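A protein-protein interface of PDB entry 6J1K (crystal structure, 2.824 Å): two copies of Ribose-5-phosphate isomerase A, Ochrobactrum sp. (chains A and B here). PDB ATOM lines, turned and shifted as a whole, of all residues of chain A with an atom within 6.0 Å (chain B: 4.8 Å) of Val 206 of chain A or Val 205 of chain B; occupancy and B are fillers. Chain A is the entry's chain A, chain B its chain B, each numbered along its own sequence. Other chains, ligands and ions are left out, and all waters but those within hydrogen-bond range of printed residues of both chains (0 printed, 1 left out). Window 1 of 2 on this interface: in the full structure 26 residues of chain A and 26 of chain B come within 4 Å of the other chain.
CD2 of Leu 104 of chain A touches OD1 of Asn 139 of chain B, at 3.6 Å. Pro 203 of chain B touches Leu 104 of chain A. Asn 139 of chain B touches His 179 of chain A (OD1 to CE1, 3.1 Å). CE2 of Phe 200 of chain A touches O of Phe 200 of chain B (3.5 Å). Pro 203 of chain A touches Glu 207 of chain B (O to OE1, 3.6 Å). Val 205 of chain A touches Val 206 of chain B (O to O, 3.9 Å). Val 205 of chain B touches Val 206 of chain A. OE1 of Glu 207 of chain A touches O of Ile 202 of chain B, 3.97 Å away. Pro 203 of chain B touches Glu 207 of chain A (CA to OE1, 3.4 Å).
Hydrophobic or aromatic side chains of chain A within 4 Å of the printed part of chain B: Leu 104, His 179 and Phe 200. Printed residues of chain B that touch a printed residue of chain A: Asn 139, Phe 200, Ile 202, Pro 203, Val 205, Val 206 and Glu 207. Hydrophobic or aromatic side chains of chain B within 4 Å of the printed part of chain A: Phe 200.
Phe 200 of chain A touches its own counterpart, Phe 200 of chain B. Pro 203 of chain A touches Glu 207 of chain B, and with the chains exchanged Glu 207 of chain A touches Pro 203 of chain B. Val 205 of chain A touches Val 206 of chain B, and with the chains exchanged Val 206 of chain A touches Val 205 of chain B. Glu 207 of chain A touches Ile 202 of chain B, but with the chains exchanged Ile 202 of chain A does not touch Glu 207 of chain B (4.2 Å). Of the 9 pairs that touch across the chains among the printed residues, 5 have their exchanged pair printed and touching as well.
The side-chain carboxylate of Glu 137 of chain A lies within hydrogen-bond range of a ring nitrogen (ND1) of His 179 of chain A. O of Glu 137 of chain A lies within hydrogen-bond range of N of Val 206 of chain A, 2.8 Å away. The backbone NH (N) of Glu 137 of chain A lies within hydrogen-bond range of the backbone carbonyl oxygen (O) of Glu 207 of chain A (2.8 Å). The backbone carbonyl oxygen (O) of Glu 137 of chain B sits at hydrogen-bond distance from the backbone NH (N) of Val 206 of chain B, 2.7 Å away. The backbone carbonyl oxygen of Glu 207 of chain B sits at hydrogen-bond distance from the backbone NH of Glu 137 of chain B (2.6 Å). The backbone carbonyl oxygen (O) of Gly 204 of chain B sits at hydrogen-bond distance from the side-chain amide nitrogen (ND2) of Asn 139 of chain B (3.0 Å).
Of chain B, only Val 205 comes within 4 Å of Val 206 of chain A. Printed residues of chain A within 4 Å of Val 206 of chain B: Val 205 (3.9 Å). Printed residues of chain B within 4 Å of Pro 203 of chain A: Glu 207 (3.6 Å). Printed residues of chain B within 4 Å of His 179 of chain A: Asn 139. Of the printed residues of chain A, Ile 202 of chain B touches Glu 207 (3.97 Å). Printed residues of chain A within 4 Å of Phe 200 of chain B: Phe 200. The nearest printed residue of chain A that does not touch Asn 139 of chain B is Val 206 of chain A (4.3 Å).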
ATOM      1  N   LEU A 104      -6.392 -20.973  -1.217  1.00  0.00           N
ATOM      2  CA  LEU A 104      -5.707 -21.181  -2.486  1.00  0.00           C
ATOM      3  C   LEU A 104      -5.414 -19.851  -3.163  1.00  0.00           C
ATOM      4  O   LEU A 104      -4.249 -19.532  -3.437  1.00  0.00           O
ATOM      5  CB  LEU A 104      -6.552 -22.064  -3.396  1.00  0.00           C
ATOM      6  CG  LEU A 104      -5.959 -22.389  -4.761  1.00  0.00           C
ATOM      7  CD1 LEU A 104      -4.578 -22.979  -4.629  1.00  0.00           C
ATOM      8  CD2 LEU A 104      -6.855 -23.372  -5.423  1.00  0.00           C
ATOM      9  N   VAL A 136      -7.026 -28.351   4.105  1.00  0.00           N
ATOM     10  CA  VAL A 136      -6.376 -28.960   2.948  1.00  0.00           C
ATOM     11  C   VAL A 136      -7.356 -28.903   1.779  1.00  0.00           C
ATOM     12  O   VAL A 136      -8.481 -29.410   1.887  1.00  0.00           O
ATOM     13  CB  VAL A 136      -5.935 -30.415   3.215  1.00  0.00           C
ATOM     14  CG1 VAL A 136      -5.371 -31.033   1.939  1.00  0.00           C
ATOM     15  CG2 VAL A 136      -4.907 -30.460   4.305  1.00  0.00           C
ATOM     16  N   GLU A 137      -6.943 -28.272   0.670  1.00  0.00           N
ATOM     17  CA  GLU A 137      -7.795 -28.128  -0.509  1.00  0.00           C
ATOM     18  C   GLU A 137      -7.563 -29.317  -1.436  1.00  0.00           C
ATOM     19  O   GLU A 137      -6.423 -29.589  -1.833  1.00  0.00           O
ATOM     20  CB  GLU A 137      -7.529 -26.812  -1.240  1.00  0.00           C
ATOM     21  CG  GLU A 137      -8.524 -26.525  -2.366  1.00  0.00           C
ATOM     22  CD  GLU A 137      -8.794 -25.044  -2.604  1.00  0.00           C
ATOM     23  OE1 GLU A 137      -8.661 -24.234  -1.654  1.00  0.00           O
ATOM     24  OE2 GLU A 137      -9.147 -24.686  -3.754  1.00  0.00           O
ATOM     25  N   VAL A 138      -8.639 -30.045  -1.744  1.00  0.00           N
ATOM     26  CA  VAL A 138      -8.577 -31.339  -2.422  1.00  0.00           C
ATOM     27  C   VAL A 138      -9.500 -31.353  -3.645  1.00  0.00           C
ATOM     28  O   VAL A 138     -10.481 -30.607  -3.721  1.00  0.00           O
ATOM     29  CB  VAL A 138      -8.920 -32.481  -1.446  1.00  0.00           C
ATOM     30  CG1 VAL A 138      -8.005 -32.446  -0.228  1.00  0.00           C
ATOM     31  CG2 VAL A 138     -10.377 -32.395  -0.992  1.00  0.00           C
ATOM     32  N   ASN A 139      -9.156 -32.185  -4.624  1.00  0.00           N
ATOM     33  CA  ASN A 139      -9.967 -32.353  -5.826  1.00  0.00           C
ATOM     34  C   ASN A 139     -11.189 -33.205  -5.507  1.00  0.00           C
ATOM     35  O   ASN A 139     -11.148 -34.102  -4.661  1.00  0.00           O
ATOM     36  CB  ASN A 139      -9.137 -33.025  -6.938  1.00  0.00           C
ATOM     37  CG  ASN A 139      -7.973 -32.160  -7.438  1.00  0.00           C
ATOM     38  OD1 ASN A 139      -8.149 -31.313  -8.309  1.00  0.00           O
ATOM     39  ND2 ASN A 139      -6.782 -32.379  -6.885  1.00  0.00           N
ATOM     40  N   HIS A 179     -12.912 -26.602  -5.633  1.00  0.00           N
ATOM     41  CA  HIS A 179     -12.361 -27.699  -4.848  1.00  0.00           C
ATOM     42  C   HIS A 179     -13.086 -27.823  -3.512  1.00  0.00           C
ATOM     43  O   HIS A 179     -13.844 -26.932  -3.100  1.00  0.00           O
ATOM     44  CB  HIS A 179     -10.872 -27.473  -4.611  1.00  0.00           C
ATOM     45  CG  HIS A 179     -10.103 -27.171  -5.858  1.00  0.00           C
ATOM     46  ND1 HIS A 179      -9.240 -26.100  -5.957  1.00  0.00           N
ATOM     47  CD2 HIS A 179     -10.037 -27.821  -7.042  1.00  0.00           C
ATOM     48  CE1 HIS A 179      -8.688 -26.091  -7.154  1.00  0.00           C
ATOM     49  NE2 HIS A 179      -9.148 -27.130  -7.828  1.00  0.00           N
ATOM     50  N   PHE A 200       1.759 -32.439  -0.381  1.00  0.00           N
ATOM     51  CA  PHE A 200       1.894 -32.184  -1.817  1.00  0.00           C
ATOM     52  C   PHE A 200       2.084 -33.475  -2.586  1.00  0.00           C
ATOM     53  O   PHE A 200       1.709 -33.559  -3.754  1.00  0.00           O
ATOM     54  CB  PHE A 200       3.066 -31.249  -2.141  1.00  0.00           C
ATOM     55  CG  PHE A 200       2.825 -29.801  -1.818  1.00  0.00           C
ATOM     56  CD1 PHE A 200       1.536 -29.260  -1.723  1.00  0.00           C
ATOM     57  CD2 PHE A 200       3.921 -28.953  -1.639  1.00  0.00           C
ATOM     58  CE1 PHE A 200       1.343 -27.872  -1.415  1.00  0.00           C
ATOM     59  CE2 PHE A 200       3.738 -27.584  -1.344  1.00  0.00           C
ATOM     60  CZ  PHE A 200       2.448 -27.049  -1.229  1.00  0.00           C
ATOM     61  N   ILE A 202       0.548 -36.043  -2.435  1.00  0.00           N
ATOM     62  CA  ILE A 202      -0.738 -36.665  -2.723  1.00  0.00           C
ATOM     63  C   ILE A 202      -1.289 -36.051  -4.004  1.00  0.00           C
ATOM     64  O   ILE A 202      -1.546 -34.833  -4.043  1.00  0.00           O
ATOM     65  CB  ILE A 202      -1.701 -36.476  -1.536  1.00  0.00           C
ATOM     66  CG1 ILE A 202      -1.104 -37.100  -0.270  1.00  0.00           C
ATOM     67  CG2 ILE A 202      -3.053 -37.090  -1.844  1.00  0.00           C
ATOM     68  CD1 ILE A 202      -1.754 -36.653   0.998  1.00  0.00           C
ATOM     69  N   PRO A 203      -1.498 -36.831  -5.068  1.00  0.00           N
ATOM     70  CA  PRO A 203      -2.031 -36.227  -6.310  1.00  0.00           C
ATOM     71  C   PRO A 203      -3.374 -35.533  -6.115  1.00  0.00           C
ATOM     72  O   PRO A 203      -3.659 -34.542  -6.805  1.00  0.00           O
ATOM     73  CB  PRO A 203      -2.101 -37.413  -7.280  1.00  0.00           C
ATOM     74  CG  PRO A 203      -1.127 -38.438  -6.706  1.00  0.00           C
ATOM     75  CD  PRO A 203      -1.247 -38.274  -5.202  1.00  0.00           C
ATOM     76  N   GLY A 204      -4.199 -36.013  -5.174  1.00  0.00           N
ATOM     77  CA  GLY A 204      -5.478 -35.394  -4.839  1.00  0.00           C
ATOM     78  C   GLY A 204      -5.395 -34.025  -4.174  1.00  0.00           C
ATOM     79  O   GLY A 204      -6.367 -33.257  -4.235  1.00  0.00           O
ATOM     80  N   VAL A 205      -4.274 -33.703  -3.534  1.00  0.00           N
ATOM     81  CA  VAL A 205      -4.130 -32.430  -2.831  1.00  0.00           C
ATOM     82  C   VAL A 205      -3.781 -31.313  -3.807  1.00  0.00           C
ATOM     83  O   VAL A 205      -2.812 -31.414  -4.564  1.00  0.00           O
ATOM     84  CB  VAL A 205      -3.084 -32.530  -1.718  1.00  0.00           C
ATOM     85  CG1 VAL A 205      -2.916 -31.177  -1.069  1.00  0.00           C
ATOM     86  CG2 VAL A 205      -3.501 -33.568  -0.718  1.00  0.00           C
ATOM     87  N   VAL A 206      -4.604 -30.259  -3.804  1.00  0.00           N
ATOM     88  CA  VAL A 206      -4.397 -29.075  -4.636  1.00  0.00           C
ATOM     89  C   VAL A 206      -3.482 -28.092  -3.932  1.00  0.00           C
ATOM     90  O   VAL A 206      -2.574 -27.509  -4.543  1.00  0.00           O
ATOM     91  CB  VAL A 206      -5.749 -28.420  -4.981  1.00  0.00           C
ATOM     92  CG1 VAL A 206      -5.530 -27.046  -5.677  1.00  0.00           C
ATOM     93  CG2 VAL A 206      -6.614 -29.349  -5.814  1.00  0.00           C
ATOM     94  N   GLU A 207      -3.740 -27.884  -2.645  1.00  0.00           N
ATOM     95  CA  GLU A 207      -2.953 -26.979  -1.820  1.00  0.00           C
ATOM     96  C   GLU A 207      -3.401 -27.154  -0.364  1.00  0.00           C
ATOM     97  O   GLU A 207      -4.310 -27.931  -0.057  1.00  0.00           O
ATOM     98  CB  GLU A 207      -3.111 -25.538  -2.321  1.00  0.00           C
ATOM     99  CG  GLU A 207      -1.899 -24.989  -3.117  1.00  0.00           C
ATOM    100  CD  GLU A 207      -0.621 -24.899  -2.285  1.00  0.00           C
ATOM    101  OE1 GLU A 207       0.467 -24.812  -2.891  1.00  0.00           O
ATOM    102  OE2 GLU A 207      -0.700 -24.920  -1.034  1.00  0.00           O
ATOM    103  N   HIS A 208      -2.737 -26.441   0.536  1.00  0.00           N
ATOM    104  CA  HIS A 208      -3.047 -26.551   1.949  1.00  0.00           C
ATOM    105  C   HIS A 208      -2.689 -25.237   2.638  1.00  0.00           C
ATOM    106  O   HIS A 208      -1.922 -24.423   2.125  1.00  0.00           O
ATOM    107  CB  HIS A 208      -2.315 -27.747   2.582  1.00  0.00           C
ATOM    108  CG  HIS A 208      -0.816 -27.692   2.428  1.00  0.00           C
ATOM    109  ND1 HIS A 208      -0.044 -26.681   2.967  1.00  0.00           N
ATOM    110  CD2 HIS A 208       0.050 -28.533   1.811  1.00  0.00           C
ATOM    111  CE1 HIS A 208       1.227 -26.894   2.674  1.00  0.00           C
ATOM    112  NE2 HIS A 208       1.312 -28.014   1.978  1.00  0.00           N
ATOM    113  N   VAL B 136       1.458 -29.371 -17.149  1.00  0.00           N
ATOM    114  CA  VAL B 136       1.317 -28.847 -15.795  1.00  0.00           C
ATOM    115  C   VAL B 136      -0.094 -28.283 -15.625  1.00  0.00           C
ATOM    116  O   VAL B 136      -0.520 -27.388 -16.370  1.00  0.00           O
ATOM    117  CB  VAL B 136       2.377 -27.785 -15.493  1.00  0.00           C
ATOM    118  CG1 VAL B 136       2.202 -27.264 -14.071  1.00  0.00           C
ATOM    119  CG2 VAL B 136       3.765 -28.381 -15.728  1.00  0.00           C
ATOM    120  N   GLU B 137      -0.814 -28.826 -14.655  1.00  0.00           N
ATOM    121  CA  GLU B 137      -2.210 -28.508 -14.439  1.00  0.00           C
ATOM    122  C   GLU B 137      -2.314 -27.344 -13.461  1.00  0.00           C
ATOM    123  O   GLU B 137      -1.787 -27.401 -12.347  1.00  0.00           O
ATOM    124  CB  GLU B 137      -2.920 -29.757 -13.916  1.00  0.00           C
ATOM    125  CG  GLU B 137      -4.442 -29.641 -13.792  1.00  0.00           C
ATOM    126  CD  GLU B 137      -5.195 -30.930 -14.101  1.00  0.00           C
ATOM    127  OE1 GLU B 137      -6.241 -31.159 -13.467  1.00  0.00           O
ATOM    128  OE2 GLU B 137      -4.762 -31.708 -14.981  1.00  0.00           O
ATOM    129  N   VAL B 138      -2.981 -26.273 -13.892  1.00  0.00           N
ATOM    130  CA  VAL B 138      -3.026 -25.015 -13.156  1.00  0.00           C
ATOM    131  C   VAL B 138      -4.463 -24.554 -12.962  1.00  0.00           C
ATOM    132  O   VAL B 138      -5.367 -24.882 -13.737  1.00  0.00           O
ATOM    133  CB  VAL B 138      -2.231 -23.919 -13.856  1.00  0.00           C
ATOM    134  CG1 VAL B 138      -0.768 -24.353 -14.043  1.00  0.00           C
ATOM    135  CG2 VAL B 138      -2.908 -23.616 -15.200  1.00  0.00           C
ATOM    136  N   ASN B 139      -4.647 -23.774 -11.897  1.00  0.00           N
ATOM    137  CA  ASN B 139      -5.911 -23.101 -11.635  1.00  0.00           C
ATOM    138  C   ASN B 139      -6.039 -21.934 -12.602  1.00  0.00           C
ATOM    139  O   ASN B 139      -5.030 -21.320 -12.981  1.00  0.00           O
ATOM    140  CB  ASN B 139      -5.948 -22.571 -10.188  1.00  0.00           C
ATOM    141  CG  ASN B 139      -5.795 -23.672  -9.119  1.00  0.00           C
ATOM    142  OD1 ASN B 139      -6.748 -24.403  -8.836  1.00  0.00           O
ATOM    143  ND2 ASN B 139      -4.603 -23.776  -8.517  1.00  0.00           N
ATOM    144  N   THR B 146       1.244 -17.567 -12.218  1.00  0.00           N
ATOM    145  CA  THR B 146       1.666 -18.966 -12.256  1.00  0.00           C
ATOM    146  C   THR B 146       2.637 -19.251 -13.405  1.00  0.00           C
ATOM    147  O   THR B 146       3.571 -20.056 -13.245  1.00  0.00           O
ATOM    148  CB  THR B 146       0.436 -19.863 -12.282  1.00  0.00           C
ATOM    149  OG1 THR B 146      -0.252 -19.699 -11.033  1.00  0.00           O
ATOM    150  CG2 THR B 146       0.809 -21.329 -12.431  1.00  0.00           C
ATOM    151  N   ILE B 150       6.401 -20.663 -12.933  1.00  0.00           N
ATOM    152  CA  ILE B 150       6.906 -21.854 -13.597  1.00  0.00           C
ATOM    153  C   ILE B 150       8.243 -21.577 -14.281  1.00  0.00           C
ATOM    154  O   ILE B 150       9.143 -22.423 -14.248  1.00  0.00           O
ATOM    155  CB  ILE B 150       5.866 -22.413 -14.583  1.00  0.00           C
ATOM    156  CG1 ILE B 150       4.680 -23.038 -13.846  1.00  0.00           C
ATOM    157  CG2 ILE B 150       6.507 -23.437 -15.469  1.00  0.00           C
ATOM    158  CD1 ILE B 150       3.538 -23.385 -14.758  1.00  0.00           C
ATOM    159  N   LEU B 199       7.865 -27.264  -8.842  1.00  0.00           N
ATOM    160  CA  LEU B 199       6.544 -26.913  -9.354  1.00  0.00           C
ATOM    161  C   LEU B 199       5.471 -26.958  -8.260  1.00  0.00           C
ATOM    162  O   LEU B 199       4.617 -26.063  -8.187  1.00  0.00           O
ATOM    163  CB  LEU B 199       6.195 -27.830 -10.530  1.00  0.00           C
ATOM    164  CG  LEU B 199       7.061 -27.744 -11.807  1.00  0.00           C
ATOM    165  CD1 LEU B 199       6.747 -28.897 -12.759  1.00  0.00           C
ATOM    166  CD2 LEU B 199       6.913 -26.409 -12.539  1.00  0.00           C
ATOM    167  N   PHE B 200       5.530 -27.959  -7.369  1.00  0.00           N
ATOM    168  CA  PHE B 200       4.597 -28.021  -6.246  1.00  0.00           C
ATOM    169  C   PHE B 200       4.693 -26.813  -5.317  1.00  0.00           C
ATOM    170  O   PHE B 200       3.704 -26.479  -4.654  1.00  0.00           O
ATOM    171  CB  PHE B 200       4.819 -29.286  -5.430  1.00  0.00           C
ATOM    172  CG  PHE B 200       4.326 -30.536  -6.089  1.00  0.00           C
ATOM    173  CD1 PHE B 200       3.318 -30.486  -7.032  1.00  0.00           C
ATOM    174  CD2 PHE B 200       4.841 -31.784  -5.729  1.00  0.00           C
ATOM    175  CE1 PHE B 200       2.845 -31.673  -7.642  1.00  0.00           C
ATOM    176  CE2 PHE B 200       4.375 -32.953  -6.329  1.00  0.00           C
ATOM    177  CZ  PHE B 200       3.383 -32.899  -7.285  1.00  0.00           C
ATOM    178  N   ILE B 202       4.791 -23.882  -6.115  1.00  0.00           N
ATOM    179  CA  ILE B 202       3.973 -22.834  -6.712  1.00  0.00           C
ATOM    180  C   ILE B 202       2.538 -23.105  -6.284  1.00  0.00           C
ATOM    181  O   ILE B 202       2.053 -24.225  -6.483  1.00  0.00           O
ATOM    182  CB  ILE B 202       4.119 -22.799  -8.241  1.00  0.00           C
ATOM    183  CG1 ILE B 202       5.568 -22.621  -8.635  1.00  0.00           C
ATOM    184  CG2 ILE B 202       3.381 -21.625  -8.848  1.00  0.00           C
ATOM    185  CD1 ILE B 202       5.829 -22.992 -10.050  1.00  0.00           C
ATOM    186  N   PRO B 203       1.880 -22.169  -5.606  1.00  0.00           N
ATOM    187  CA  PRO B 203       0.472 -22.385  -5.217  1.00  0.00           C
ATOM    188  C   PRO B 203      -0.494 -22.599  -6.382  1.00  0.00           C
ATOM    189  O   PRO B 203      -1.448 -23.386  -6.266  1.00  0.00           O
ATOM    190  CB  PRO B 203       0.142 -21.113  -4.424  1.00  0.00           C
ATOM    191  CG  PRO B 203       1.494 -20.584  -3.945  1.00  0.00           C
ATOM    192  CD  PRO B 203       2.439 -20.916  -5.069  1.00  0.00           C
ATOM    193  N   GLY B 204      -0.264 -21.933  -7.514  1.00  0.00           N
ATOM    194  CA  GLY B 204      -1.126 -22.107  -8.669  1.00  0.00           C
ATOM    195  C   GLY B 204      -1.064 -23.485  -9.271  1.00  0.00           C
ATOM    196  O   GLY B 204      -1.978 -23.881  -9.999  1.00  0.00           O
ATOM    197  N   VAL B 205       0.001 -24.228  -8.999  1.00  0.00           N
ATOM    198  CA  VAL B 205       0.157 -25.533  -9.619  1.00  0.00           C
ATOM    199  C   VAL B 205      -0.711 -26.560  -8.904  1.00  0.00           C
ATOM    200  O   VAL B 205      -0.645 -26.725  -7.680  1.00  0.00           O
ATOM    201  CB  VAL B 205       1.633 -25.926  -9.650  1.00  0.00           C
ATOM    202  CG1 VAL B 205       1.784 -27.389  -9.961  1.00  0.00           C
ATOM    203  CG2 VAL B 205       2.334 -25.056 -10.685  1.00  0.00           C
ATOM    204  N   VAL B 206      -1.574 -27.213  -9.669  1.00  0.00           N
ATOM    205  CA  VAL B 206      -2.431 -28.261  -9.131  1.00  0.00           C
ATOM    206  C   VAL B 206      -1.703 -29.600  -9.116  1.00  0.00           C
ATOM    207  O   VAL B 206      -1.744 -30.340  -8.119  1.00  0.00           O
ATOM    208  CB  VAL B 206      -3.726 -28.322  -9.951  1.00  0.00           C
ATOM    209  CG1 VAL B 206      -4.532 -29.553  -9.554  1.00  0.00           C
ATOM    210  CG2 VAL B 206      -4.504 -26.996  -9.785  1.00  0.00           C
ATOM    211  N   GLU B 207      -1.062 -29.939 -10.243  1.00  0.00           N
ATOM    212  CA  GLU B 207      -0.288 -31.163 -10.417  1.00  0.00           C
ATOM    213  C   GLU B 207       0.334 -31.106 -11.811  1.00  0.00           C
ATOM    214  O   GLU B 207       0.043 -30.157 -12.547  1.00  0.00           O
ATOM    215  CB  GLU B 207      -1.145 -32.419 -10.207  1.00  0.00           C
ATOM    216  CG  GLU B 207      -0.295 -33.667 -10.029  1.00  0.00           C
ATOM    217  CD  GLU B 207       0.058 -33.902  -8.581  1.00  0.00           C
ATOM    218  OE1 GLU B 207      -0.449 -33.150  -7.715  1.00  0.00           O
ATOM    219  OE2 GLU B 207       0.880 -34.785  -8.311  1.00  0.00           O
